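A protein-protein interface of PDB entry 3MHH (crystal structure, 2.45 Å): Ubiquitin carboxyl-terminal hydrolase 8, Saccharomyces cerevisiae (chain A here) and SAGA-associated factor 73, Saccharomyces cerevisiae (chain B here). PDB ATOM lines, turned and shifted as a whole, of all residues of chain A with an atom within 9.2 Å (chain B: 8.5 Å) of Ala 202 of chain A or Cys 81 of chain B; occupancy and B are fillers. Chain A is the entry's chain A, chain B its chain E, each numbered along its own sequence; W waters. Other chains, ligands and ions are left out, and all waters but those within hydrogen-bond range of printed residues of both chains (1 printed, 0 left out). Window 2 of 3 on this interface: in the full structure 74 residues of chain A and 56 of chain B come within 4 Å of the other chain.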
ATOM      1  N   LYS A 129      -4.573 -18.412  14.833  1.00  0.00           N
ATOM      2  CA  LYS A 129      -5.431 -19.097  13.867  1.00  0.00           C
ATOM      3  C   LYS A 129      -6.806 -19.488  14.411  1.00  0.00           C
ATOM      4  O   LYS A 129      -7.673 -19.938  13.657  1.00  0.00           O
ATOM      5  CB  LYS A 129      -4.713 -20.334  13.335  1.00  0.00           C
ATOM      6  CG  LYS A 129      -3.485 -20.002  12.502  1.00  0.00           C
ATOM      7  CD  LYS A 129      -2.684 -21.251  12.154  1.00  0.00           C
ATOM      8  CE  LYS A 129      -1.520 -20.920  11.218  1.00  0.00           C
ATOM      9  NZ  LYS A 129      -1.096 -22.107  10.424  1.00  0.00           N
ATOM     10  N   THR A 130      -6.997 -19.319  15.717  1.00  0.00           N
ATOM     11  CA  THR A 130      -8.267 -19.607  16.354  1.00  0.00           C
ATOM     12  C   THR A 130      -8.574 -18.509  17.363  1.00  0.00           C
ATOM     13  O   THR A 130      -7.668 -17.886  17.912  1.00  0.00           O
ATOM     14  CB  THR A 130      -8.233 -20.968  17.097  1.00  0.00           C
ATOM     15  OG1 THR A 130      -7.431 -20.858  18.286  1.00  0.00           O
ATOM     16  CG2 THR A 130      -7.684 -22.078  16.186  1.00  0.00           C
ATOM     17  N   MET A 131      -9.859 -18.297  17.622  1.00  0.00           N
ATOM     18  CA  MET A 131     -10.299 -17.248  18.528  1.00  0.00           C
ATOM     19  C   MET A 131     -11.221 -17.840  19.588  1.00  0.00           C
ATOM     20  O   MET A 131     -11.792 -18.911  19.393  1.00  0.00           O
ATOM     21  CB  MET A 131     -11.042 -16.168  17.746  1.00  0.00           C
ATOM     22  CG  MET A 131     -12.345 -16.648  17.119  1.00  0.00           C
ATOM     23  SD  MET A 131     -13.082 -15.479  15.939  1.00  0.00           S
ATOM     24  CE  MET A 131     -14.820 -15.957  16.055  1.00  0.00           C
ATOM     25  N   VAL A 132     -11.370 -17.140  20.704  1.00  0.00           N
ATOM     26  CA  VAL A 132     -12.265 -17.593  21.763  1.00  0.00           C
ATOM     27  C   VAL A 132     -13.706 -17.512  21.251  1.00  0.00           C
ATOM     28  O   VAL A 132     -13.979 -16.830  20.280  1.00  0.00           O
ATOM     29  CB  VAL A 132     -12.095 -16.738  23.046  1.00  0.00           C
ATOM     30  CG1 VAL A 132     -10.609 -16.691  23.455  1.00  0.00           C
ATOM     31  CG2 VAL A 132     -12.637 -15.307  22.820  1.00  0.00           C
ATOM     32  N   PRO A 133     -14.630 -18.239  21.885  1.00  0.00           N
ATOM     33  CA  PRO A 133     -16.007 -18.190  21.396  1.00  0.00           C
ATOM     34  C   PRO A 133     -16.616 -16.800  21.509  1.00  0.00           C
ATOM     35  O   PRO A 133     -16.250 -16.028  22.393  1.00  0.00           O
ATOM     36  CB  PRO A 133     -16.748 -19.164  22.320  1.00  0.00           C
ATOM     37  CG  PRO A 133     -15.688 -20.042  22.891  1.00  0.00           C
ATOM     38  CD  PRO A 133     -14.473 -19.176  23.007  1.00  0.00           C
ATOM     39  N   SER A 134     -17.551 -16.486  20.626  1.00  0.00           N
ATOM     40  CA  SER A 134     -18.244 -15.232  20.747  1.00  0.00           C
ATOM     41  C   SER A 134     -19.206 -15.326  21.919  1.00  0.00           C
ATOM     42  O   SER A 134     -19.708 -16.398  22.245  1.00  0.00           O
ATOM     43  CB  SER A 134     -18.968 -14.867  19.452  1.00  0.00           C
ATOM     44  OG  SER A 134     -20.188 -15.560  19.342  1.00  0.00           O
ATOM     45  N   ARG A 137     -22.559 -17.184  21.280  1.00  0.00           N
ATOM     46  CA  ARG A 137     -22.601 -18.592  20.885  1.00  0.00           C
ATOM     47  C   ARG A 137     -21.941 -19.494  21.917  1.00  0.00           C
ATOM     48  O   ARG A 137     -21.995 -20.713  21.794  1.00  0.00           O
ATOM     49  CB  ARG A 137     -21.878 -18.777  19.550  1.00  0.00           C
ATOM     50  CG  ARG A 137     -22.376 -17.894  18.427  1.00  0.00           C
ATOM     51  CD  ARG A 137     -23.720 -18.374  17.856  1.00  0.00           C
ATOM     52  NE  ARG A 137     -24.850 -17.609  18.386  1.00  0.00           N
ATOM     53  CZ  ARG A 137     -25.809 -18.104  19.169  1.00  0.00           C
ATOM     54  NH1 ARG A 137     -25.815 -19.395  19.511  1.00  0.00           N
ATOM     55  NH2 ARG A 137     -26.798 -17.311  19.572  1.00  0.00           N
ATOM     56  N   GLN A 173     -13.895 -33.384  16.038  1.00  0.00           N
ATOM     57  CA  GLN A 173     -13.725 -33.624  14.593  1.00  0.00           C
ATOM     58  C   GLN A 173     -13.612 -35.097  14.206  1.00  0.00           C
ATOM     59  O   GLN A 173     -13.297 -35.426  13.054  1.00  0.00           O
ATOM     60  CB  GLN A 173     -12.524 -32.851  14.043  1.00  0.00           C
ATOM     61  CG  GLN A 173     -12.525 -31.377  14.401  1.00  0.00           C
ATOM     62  CD  GLN A 173     -13.768 -30.670  13.925  1.00  0.00           C
ATOM     63  OE1 GLN A 173     -14.496 -30.062  14.721  1.00  0.00           O
ATOM     64  NE2 GLN A 173     -14.054 -30.784  12.634  1.00  0.00           N
ATOM     65  N   SER A 176     -15.836 -35.859  11.215  1.00  0.00           N
ATOM     66  CA  SER A 176     -15.418 -35.094  10.037  1.00  0.00           C
ATOM     67  C   SER A 176     -14.132 -35.646   9.439  1.00  0.00           C
ATOM     68  O   SER A 176     -13.922 -35.577   8.230  1.00  0.00           O
ATOM     69  CB  SER A 176     -15.213 -33.621  10.400  1.00  0.00           C
ATOM     70  OG  SER A 176     -14.760 -32.892   9.271  1.00  0.00           O
ATOM     71  N   LYS A 194     -22.921 -29.741  11.560  1.00  0.00           N
ATOM     72  CA  LYS A 194     -23.172 -28.407  11.063  1.00  0.00           C
ATOM     73  C   LYS A 194     -24.011 -27.602  12.043  1.00  0.00           C
ATOM     74  O   LYS A 194     -23.812 -26.404  12.198  1.00  0.00           O
ATOM     75  CB  LYS A 194     -23.848 -28.461   9.695  1.00  0.00           C
ATOM     76  CG  LYS A 194     -24.028 -27.100   9.069  1.00  0.00           C
ATOM     77  CD  LYS A 194     -23.429 -27.049   7.655  1.00  0.00           C
ATOM     78  CE  LYS A 194     -21.919 -27.328   7.667  1.00  0.00           C
ATOM     79  NZ  LYS A 194     -21.241 -26.766   6.462  1.00  0.00           N
ATOM     80  N   ILE A 195     -24.950 -28.261  12.706  1.00  0.00           N
ATOM     81  CA  ILE A 195     -25.754 -27.598  13.716  1.00  0.00           C
ATOM     82  C   ILE A 195     -24.869 -27.102  14.855  1.00  0.00           C
ATOM     83  O   ILE A 195     -25.023 -25.981  15.337  1.00  0.00           O
ATOM     84  CB  ILE A 195     -26.822 -28.540  14.302  1.00  0.00           C
ATOM     85  CG1 ILE A 195     -27.780 -28.992  13.193  1.00  0.00           C
ATOM     86  CG2 ILE A 195     -27.572 -27.824  15.393  1.00  0.00           C
ATOM     87  CD1 ILE A 195     -28.671 -30.155  13.582  1.00  0.00           C
ATOM     88  N   VAL A 196     -23.941 -27.949  15.273  1.00  0.00           N
ATOM     89  CA  VAL A 196     -23.044 -27.619  16.356  1.00  0.00           C
ATOM     90  C   VAL A 196     -22.202 -26.428  15.945  1.00  0.00           C
ATOM     91  O   VAL A 196     -21.926 -25.523  16.742  1.00  0.00           O
ATOM     92  CB  VAL A 196     -22.104 -28.804  16.666  1.00  0.00           C
ATOM     93  CG1 VAL A 196     -21.024 -28.380  17.630  1.00  0.00           C
ATOM     94  CG2 VAL A 196     -22.887 -29.952  17.214  1.00  0.00           C
ATOM     95  N   HIS A 197     -21.786 -26.465  14.687  1.00  0.00           N
ATOM     96  CA  HIS A 197     -20.994 -25.412  14.085  1.00  0.00           C
ATOM     97  C   HIS A 197     -21.774 -24.109  14.161  1.00  0.00           C
ATOM     98  O   HIS A 197     -21.248 -23.095  14.615  1.00  0.00           O
ATOM     99  CB  HIS A 197     -20.683 -25.807  12.634  1.00  0.00           C
ATOM    100  CG  HIS A 197     -19.817 -24.842  11.882  1.00  0.00           C
ATOM    101  ND1 HIS A 197     -19.181 -25.189  10.706  1.00  0.00           N
ATOM    102  CD2 HIS A 197     -19.515 -23.540  12.104  1.00  0.00           C
ATOM    103  CE1 HIS A 197     -18.516 -24.145  10.244  1.00  0.00           C
ATOM    104  NE2 HIS A 197     -18.709 -23.130  11.066  1.00  0.00           N
ATOM    105  N   GLU A 198     -23.045 -24.147  13.772  1.00  0.00           N
ATOM    106  CA  GLU A 198     -23.873 -22.935  13.750  1.00  0.00           C
ATOM    107  C   GLU A 198     -24.153 -22.384  15.144  1.00  0.00           C
ATOM    108  O   GLU A 198     -24.285 -21.174  15.334  1.00  0.00           O
ATOM    109  CB  GLU A 198     -25.226 -23.229  13.116  1.00  0.00           C
ATOM    110  CG  GLU A 198     -25.240 -23.336  11.626  1.00  0.00           C
ATOM    111  CD  GLU A 198     -26.650 -23.470  11.105  1.00  0.00           C
ATOM    112  OE1 GLU A 198     -27.241 -24.547  11.327  1.00  0.00           O
ATOM    113  OE2 GLU A 198     -27.169 -22.498  10.498  1.00  0.00           O
ATOM    114  N   LEU A 199     -24.313 -23.291  16.098  1.00  0.00           N
ATOM    115  CA  LEU A 199     -24.755 -22.918  17.424  1.00  0.00           C
ATOM    116  C   LEU A 199     -23.615 -22.453  18.319  1.00  0.00           C
ATOM    117  O   LEU A 199     -23.827 -21.615  19.182  1.00  0.00           O
ATOM    118  CB  LEU A 199     -25.503 -24.082  18.082  1.00  0.00           C
ATOM    119  CG  LEU A 199     -27.013 -24.161  17.814  1.00  0.00           C
ATOM    120  CD1 LEU A 199     -27.318 -24.163  16.348  1.00  0.00           C
ATOM    121  CD2 LEU A 199     -27.607 -25.405  18.474  1.00  0.00           C
ATOM    122  N   TYR A 200     -22.414 -22.986  18.099  1.00  0.00           N
ATOM    123  CA  TYR A 200     -21.257 -22.716  18.959  1.00  0.00           C
ATOM    124  C   TYR A 200     -20.156 -21.894  18.272  1.00  0.00           C
ATOM    125  O   TYR A 200     -19.323 -21.266  18.937  1.00  0.00           O
ATOM    126  CB  TYR A 200     -20.664 -24.041  19.427  1.00  0.00           C
ATOM    127  CG  TYR A 200     -21.453 -24.728  20.516  1.00  0.00           C
ATOM    128  CD1 TYR A 200     -21.273 -24.384  21.849  1.00  0.00           C
ATOM    129  CD2 TYR A 200     -22.352 -25.737  20.219  1.00  0.00           C
ATOM    130  CE1 TYR A 200     -21.955 -25.021  22.855  1.00  0.00           C
ATOM    131  CE2 TYR A 200     -23.043 -26.378  21.213  1.00  0.00           C
ATOM    132  CZ  TYR A 200     -22.837 -26.024  22.538  1.00  0.00           C
ATOM    133  OH  TYR A 200     -23.537 -26.659  23.546  1.00  0.00           O
ATOM    134  N   GLY A 201     -20.139 -21.923  16.941  1.00  0.00           N
ATOM    135  CA  GLY A 201     -19.173 -21.145  16.165  1.00  0.00           C
ATOM    136  C   GLY A 201     -19.842 -20.202  15.179  1.00  0.00           C
ATOM    137  O   GLY A 201     -20.843 -19.561  15.507  1.00  0.00           O
ATOM    138  N   ALA A 202     -19.279 -20.111  13.975  1.00  0.00           N
ATOM    139  CA  ALA A 202     -19.794 -19.227  12.907  1.00  0.00           C
ATOM    140  C   ALA A 202     -19.762 -19.983  11.592  1.00  0.00           C
ATOM    141  O   ALA A 202     -18.714 -20.478  11.193  1.00  0.00           O
ATOM    142  CB  ALA A 202     -18.951 -17.959  12.796  1.00  0.00           C
ATOM    143  N   LEU A 203     -20.910 -20.072  10.923  1.00  0.00           N
ATOM    144  CA  LEU A 203     -21.024 -20.892   9.716  1.00  0.00           C
ATOM    145  C   LEU A 203     -20.688 -20.125   8.427  1.00  0.00           C
ATOM    146  O   LEU A 203     -20.208 -20.714   7.452  1.00  0.00           O
ATOM    147  CB  LEU A 203     -22.423 -21.505   9.625  1.00  0.00           C
ATOM    148  CG  LEU A 203     -22.532 -22.733   8.722  1.00  0.00           C
ATOM    149  CD1 LEU A 203     -21.746 -23.894   9.305  1.00  0.00           C
ATOM    150  CD2 LEU A 203     -23.983 -23.122   8.505  1.00  0.00           C
ATOM    151  N   ASN A 204     -20.917 -18.813   8.431  1.00  0.00           N
ATOM    152  CA  ASN A 204     -20.657 -17.986   7.249  1.00  0.00           C
ATOM    153  C   ASN A 204     -19.663 -16.869   7.574  1.00  0.00           C
ATOM    154  O   ASN A 204     -19.052 -16.865   8.649  1.00  0.00           O
ATOM    155  CB  ASN A 204     -21.974 -17.381   6.726  1.00  0.00           C
ATOM    156  CG  ASN A 204     -22.043 -17.344   5.200  1.00  0.00           C
ATOM    157  OD1 ASN A 204     -21.979 -16.275   4.582  1.00  0.00           O
ATOM    158  ND2 ASN A 204     -22.177 -18.518   4.587  1.00  0.00           N
ATOM    159  N   THR A 205     -19.509 -15.931   6.637  1.00  0.00           N
ATOM    160  CA  THR A 205     -18.688 -14.737   6.846  1.00  0.00           C
ATOM    161  C   THR A 205     -19.586 -13.539   7.157  1.00  0.00           C
ATOM    162  O   THR A 205     -19.435 -12.882   8.188  1.00  0.00           O
ATOM    163  CB  THR A 205     -17.837 -14.406   5.596  1.00  0.00           C
ATOM    164  OG1 THR A 205     -16.803 -13.473   5.943  1.00  0.00           O
ATOM    165  CG2 THR A 205     -18.713 -13.808   4.478  1.00  0.00           C
ATOM    166  N   ARG A 217     -29.502 -19.488  11.895  1.00  0.00           N
ATOM    167  CA  ARG A 217     -28.976 -20.729  12.449  1.00  0.00           C
ATOM    168  C   ARG A 217     -29.948 -21.896  12.303  1.00  0.00           C
ATOM    169  O   ARG A 217     -30.119 -22.683  13.229  1.00  0.00           O
ATOM    170  CB  ARG A 217     -28.587 -20.542  13.926  1.00  0.00           C
ATOM    171  CG  ARG A 217     -27.398 -19.586  14.151  1.00  0.00           C
ATOM    172  CD  ARG A 217     -27.067 -19.404  15.654  1.00  0.00           C
ATOM    173  NE  ARG A 217     -28.152 -18.703  16.329  1.00  0.00           N
ATOM    174  CZ  ARG A 217     -28.283 -17.380  16.361  1.00  0.00           C
ATOM    175  NH1 ARG A 217     -27.375 -16.604  15.797  1.00  0.00           N
ATOM    176  NH2 ARG A 217     -29.322 -16.830  16.963  1.00  0.00           N
ATOM    177  N   TYR B  75     -13.515 -24.509  24.298  1.00  0.00           N
ATOM    178  CA  TYR B  75     -13.188 -24.632  22.883  1.00  0.00           C
ATOM    179  C   TYR B  75     -12.726 -23.321  22.294  1.00  0.00           C
ATOM    180  O   TYR B  75     -12.781 -22.281  22.947  1.00  0.00           O
ATOM    181  CB  TYR B  75     -14.379 -25.160  22.086  1.00  0.00           C
ATOM    182  CG  TYR B  75     -15.550 -24.201  21.971  1.00  0.00           C
ATOM    183  CD1 TYR B  75     -16.362 -23.928  23.060  1.00  0.00           C
ATOM    184  CD2 TYR B  75     -15.873 -23.620  20.754  1.00  0.00           C
ATOM    185  CE1 TYR B  75     -17.449 -23.071  22.944  1.00  0.00           C
ATOM    186  CE2 TYR B  75     -16.958 -22.769  20.625  1.00  0.00           C
ATOM    187  CZ  TYR B  75     -17.741 -22.495  21.719  1.00  0.00           C
ATOM    188  OH  TYR B  75     -18.820 -21.652  21.579  1.00  0.00           O
ATOM    189  N   VAL B  77     -12.520 -21.246  18.195  1.00  0.00           N
ATOM    190  CA  VAL B  77     -13.175 -21.211  16.897  1.00  0.00           C
ATOM    191  C   VAL B  77     -12.178 -20.866  15.809  1.00  0.00           C
ATOM    192  O   VAL B  77     -11.508 -19.843  15.869  1.00  0.00           O
ATOM    193  CB  VAL B  77     -14.330 -20.183  16.894  1.00  0.00           C
ATOM    194  CG1 VAL B  77     -14.939 -20.049  15.500  1.00  0.00           C
ATOM    195  CG2 VAL B  77     -15.381 -20.592  17.908  1.00  0.00           C
ATOM    196  N   CYS B  78     -12.075 -21.736  14.817  1.00  0.00           N
ATOM    197  CA  CYS B  78     -11.173 -21.517  13.693  1.00  0.00           C
ATOM    198  C   CYS B  78     -11.588 -20.267  12.919  1.00  0.00           C
ATOM    199  O   CYS B  78     -12.751 -20.108  12.549  1.00  0.00           O
ATOM    200  CB  CYS B  78     -11.194 -22.746  12.788  1.00  0.00           C
ATOM    201  SG  CYS B  78     -10.330 -22.575  11.223  1.00  0.00           S
ATOM    202  N   GLU B  79     -10.639 -19.369  12.690  1.00  0.00           N
ATOM    203  CA  GLU B  79     -10.952 -18.100  12.044  1.00  0.00           C
ATOM    204  C   GLU B  79     -11.102 -18.239  10.538  1.00  0.00           C
ATOM    205  O   GLU B  79     -11.610 -17.344   9.872  1.00  0.00           O
ATOM    206  CB  GLU B  79      -9.897 -17.058  12.385  1.00  0.00           C
ATOM    207  CG  GLU B  79      -9.825 -16.781  13.879  1.00  0.00           C
ATOM    208  CD  GLU B  79      -8.812 -15.724  14.225  1.00  0.00           C
ATOM    209  OE1 GLU B  79      -8.299 -15.074  13.292  1.00  0.00           O
ATOM    210  OE2 GLU B  79      -8.533 -15.543  15.431  1.00  0.00           O
ATOM    211  N   LYS B  80     -10.704 -19.391  10.019  1.00  0.00           N
ATOM    212  CA  LYS B  80     -10.817 -19.672   8.600  1.00  0.00           C
ATOM    213  C   LYS B  80     -12.213 -20.177   8.247  1.00  0.00           C
ATOM    214  O   LYS B  80     -12.876 -19.620   7.373  1.00  0.00           O
ATOM    215  CB  LYS B  80      -9.766 -20.705   8.200  1.00  0.00           C
ATOM    216  CG  LYS B  80      -9.575 -20.861   6.710  1.00  0.00           C
ATOM    217  CD  LYS B  80      -8.331 -21.687   6.396  1.00  0.00           C
ATOM    218  CE  LYS B  80      -8.315 -22.116   4.928  1.00  0.00           C
ATOM    219  NZ  LYS B  80      -8.655 -20.994   4.009  1.00  0.00           N
ATOM    220  N   CYS B  81     -12.663 -21.223   8.939  1.00  0.00           N
ATOM    221  CA  CYS B  81     -13.941 -21.855   8.613  1.00  0.00           C
ATOM    222  C   CYS B  81     -15.015 -21.682   9.692  1.00  0.00           C
ATOM    223  O   CYS B  81     -16.170 -22.031   9.479  1.00  0.00           O
ATOM    224  CB  CYS B  81     -13.736 -23.344   8.314  1.00  0.00           C
ATOM    225  SG  CYS B  81     -13.279 -24.332   9.750  1.00  0.00           S
ATOM    226  N   GLY B  82     -14.632 -21.154  10.848  1.00  0.00           N
ATOM    227  CA  GLY B  82     -15.592 -20.881  11.912  1.00  0.00           C
ATOM    228  C   GLY B  82     -16.025 -22.066  12.764  1.00  0.00           C
ATOM    229  O   GLY B  82     -16.849 -21.896  13.653  1.00  0.00           O
ATOM    230  N   LYS B  83     -15.474 -23.258  12.518  1.00  0.00           N
ATOM    231  CA  LYS B  83     -15.847 -24.453  13.292  1.00  0.00           C
ATOM    232  C   LYS B  83     -15.424 -24.338  14.746  1.00  0.00           C
ATOM    233  O   LYS B  83     -14.358 -23.820  15.042  1.00  0.00           O
ATOM    234  CB  LYS B  83     -15.200 -25.712  12.721  1.00  0.00           C
ATOM    235  CG  LYS B  83     -15.945 -26.373  11.573  1.00  0.00           C
ATOM    236  CD  LYS B  83     -15.203 -27.615  11.108  1.00  0.00           C
ATOM    237  CE  LYS B  83     -15.784 -28.158   9.812  1.00  0.00           C
ATOM    238  NZ  LYS B  83     -15.357 -29.566   9.557  1.00  0.00           N
ATOM    239  N   PRO B  84     -16.266 -24.816  15.666  1.00  0.00           N
ATOM    240  CA  PRO B  84     -15.837 -24.890  17.063  1.00  0.00           C
ATOM    241  C   PRO B  84     -14.942 -26.097  17.276  1.00  0.00           C
ATOM    242  O   PRO B  84     -15.334 -27.215  16.931  1.00  0.00           O
ATOM    243  CB  PRO B  84     -17.154 -25.053  17.830  1.00  0.00           C
ATOM    244  CG  PRO B  84     -18.071 -25.722  16.861  1.00  0.00           C
ATOM    245  CD  PRO B  84     -17.685 -25.173  15.495  1.00  0.00           C
ATOM    246  N   LEU B  85     -13.757 -25.883  17.844  1.00  0.00           N
ATOM    247  CA  LEU B  85     -12.770 -26.955  17.985  1.00  0.00           C
ATOM    248  C   LEU B  85     -12.431 -27.249  19.439  1.00  0.00           C
ATOM    249  O   LEU B  85     -12.053 -26.342  20.191  1.00  0.00           O
ATOM    250  CB  LEU B  85     -11.489 -26.558  17.259  1.00  0.00           C
ATOM    251  CG  LEU B  85     -11.580 -26.234  15.763  1.00  0.00           C
ATOM    252  CD1 LEU B  85     -10.328 -25.480  15.297  1.00  0.00           C
ATOM    253  CD2 LEU B  85     -11.767 -27.500  14.928  1.00  0.00           C
ATOM    254  N   HIS B  93      -6.298 -29.736  13.308  1.00  0.00           N
ATOM    255  CA  HIS B  93      -7.174 -29.022  12.382  1.00  0.00           C
ATOM    256  C   HIS B  93      -6.393 -27.952  11.631  1.00  0.00           C
ATOM    257  O   HIS B  93      -6.679 -27.669  10.464  1.00  0.00           O
ATOM    258  CB  HIS B  93      -8.365 -28.376  13.092  1.00  0.00           C
ATOM    259  CG  HIS B  93      -9.228 -27.560  12.178  1.00  0.00           C
ATOM    260  ND1 HIS B  93     -10.239 -28.109  11.415  1.00  0.00           N
ATOM    261  CD2 HIS B  93      -9.194 -26.242  11.864  1.00  0.00           C
ATOM    262  CE1 HIS B  93     -10.806 -27.160  10.692  1.00  0.00           C
ATOM    263  NE2 HIS B  93     -10.181 -26.020  10.935  1.00  0.00           N
ATOM    264  N   LEU B  94      -5.409 -27.360  12.308  1.00  0.00           N
ATOM    265  CA  LEU B  94      -4.572 -26.324  11.705  1.00  0.00           C
ATOM    266  C   LEU B  94      -3.570 -26.898  10.699  1.00  0.00           C
ATOM    267  O   LEU B  94      -2.919 -26.148   9.969  1.00  0.00           O
ATOM    268  CB  LEU B  94      -3.814 -25.545  12.785  1.00  0.00           C
ATOM    269  CG  LEU B  94      -4.653 -24.696  13.736  1.00  0.00           C
ATOM    270  CD1 LEU B  94      -3.749 -23.780  14.559  1.00  0.00           C
ATOM    271  CD2 LEU B  94      -5.699 -23.890  12.965  1.00  0.00           C
ATOM    272  N   ASN B  96      -4.456 -29.780   8.598  1.00  0.00           N
ATOM    273  CA  ASN B  96      -5.149 -30.372   7.452  1.00  0.00           C
ATOM    274  C   ASN B  96      -5.355 -29.369   6.311  1.00  0.00           C
ATOM    275  O   ASN B  96      -4.540 -29.299   5.387  1.00  0.00           O
ATOM    276  CB  ASN B  96      -6.472 -31.051   7.878  1.00  0.00           C
ATOM    277  CG  ASN B  96      -7.580 -30.055   8.244  1.00  0.00           C
ATOM    278  OD1 ASN B  96      -7.418 -28.840   8.117  1.00  0.00           O
ATOM    279  ND2 ASN B  96      -8.721 -30.581   8.698  1.00  0.00           N
ATOM    280  OXT ASN B  96      -6.315 -28.598   6.272  1.00  0.00           O
HETATM  281  O   HOH W   1     -16.476 -28.262  14.869  1.00  0.00           O
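The side-chain hydroxyl of Ser 134 of chain A sits close to the backbone NH of Arg 137 of chain A, 3.5 Å away.
NH1 of Arg 137 of chain A sits at hydrogen-bond distance from O of Leu 199 of chain A, 3.0 Å away.
A ring nitrogen (NE2) of His 197 of chain A sits at hydrogen-bond distance from the backbone carbonyl oxygen (O) of Ala 202 of chain A.
The side-chain sulfur (SG) of Cys 78 of chain B sits close to the backbone NH (N) of Lys 80 of chain B (3.4 Å).
The backbone carbonyl oxygen of Lys 83 of chain B sits at hydrogen-bond distance from the backbone NH of Cys 78 of chain B, 3.1 Å away.
SG of Cys 81 of chain B sits close to N of Lys 83 of chain B, at 3.7 Å.
Printed residues of chain B within 4 Å of Pro 133 of chain A: Tyr 75 (3.3 Å).
Glu 198 of chain A touches none of the printed residues of chain B.
Of chain B, only Cys 81 and Gly 82 come within 4 Å of Ala 202 of chain A.
Arg 217 of chain A touches none of the printed residues of chain B.
Of the printed residues of chain A, Val 77 of chain B touches Thr 130 (3.3 Å) and Met 131 (2.7 Å).
Printed residues of chain A within 4 Å of Cys 78 of chain B: Lys 129 (3.8 Å).
Printed residues of chain A within 4 Å of Cys 81 of chain B: His 197 (3.2 Å) and Ala 202 (3.4 Å).
Gly 82 of chain B touches just these residues of chain A: His 197 (3.3 Å), Gly 201 (3.5 Å) and Ala 202 (3.0 Å).
The nearest residue of chain B that does not touch Ala 202 of chain A is Lys 83 of chain B (4.5 Å).
The nearest residue of chain A that does not touch Cys 81 of chain B is Leu 203 of chain A (4.7 Å).
The nearest printed residue of chain A that does not touch Leu 85 of chain B is Thr 130 of chain A (4.4 Å).
Printed residues of chain A that touch a printed residue of chain B: Lys 129, Thr 130, Met 131, Pro 133, Arg 137, Gln 173, Ser 176, Val 196, His 197, Tyr 200, Gly 201 and Ala 202.
Hydrophobic or aromatic side chains of chain B that line the printed part of chain A: Tyr 75, Val 77, Pro 84, Leu 85 and Leu 94.
Lys 129 of chain A touches Cys 78 of chain B.
O of Val 77 of chain B touches CA of Thr 130 of chain A (3.3 Å).
Thr 130 of chain A touches Glu 79 of chain B (O to OE2, 3.5 Å).
CB of Met 131 of chain A touches OE2 of Glu 79 of chain B, at 3.5 Å.
CB of Pro 133 of chain A touches OH of Tyr 75 of chain B, at 3.3 Å.
O of Pro 84 of chain B touches OE1 of Gln 173 of chain A (3.7 Å).
Pro 84 of chain B touches Val 196 of chain A (CG to O, 3.9 Å).
N of Lys 83 of chain B touches NE2 of His 197 of chain A, at 3.5 Å.
CD of Pro 84 of chain B touches CA of His 197 of chain A, 3.6 Å away.
Gly 201 of chain A touches Gly 82 of chain B (CA to O, 3.5 Å).
Water W1 lies within hydrogen-bond range of the backbone carbonyl oxygen (O) of Pro 84 of chain B (2.6 Å) and the side-chain amide oxygen (OE1) of Gln 173 of chain A (2.7 Å).
O of Lys 129 of chain A lies within hydrogen-bond range of N of Glu 79 of chain B, 3.2 Å away.
The backbone carbonyl oxygen (O) of Met 131 of chain A lies within hydrogen-bond range of the backbone NH (N) of Val 77 of chain B, at 2.7 Å.
The backbone carbonyl oxygen (O) of Arg 137 of chain A is in hydrogen-bond range of the side-chain hydroxyl (OH) of Tyr 75 of chain B.
The side-chain amino group (NZ) of Lys 83 of chain B lies within hydrogen-bond range of the side-chain hydroxyl (OG) of Ser 176 of chain A (3.4 Å).
The backbone carbonyl oxygen (O) of Cys 81 of chain B is in hydrogen-bond range of a ring nitrogen (NE2) of His 197 of chain A.
A ring nitrogen (NE2) of His 197 of chain A sits close to the backbone carbonyl oxygen (O) of Gly 82 of chain B (3.4 Å).
The backbone carbonyl oxygen (O) of Tyr 200 of chain A lies within hydrogen-bond range of the side-chain hydroxyl (OH) of Tyr 75 of chain B.
O of Gly 82 of chain B lies within hydrogen-bond range of N of Ala 202 of chain A (3.0 Å).
The backbone carbonyl oxygen of Ala 202 of chain A sits close to the backbone carbonyl oxygen of Cys 81 of chain B, at 3.4 Å.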
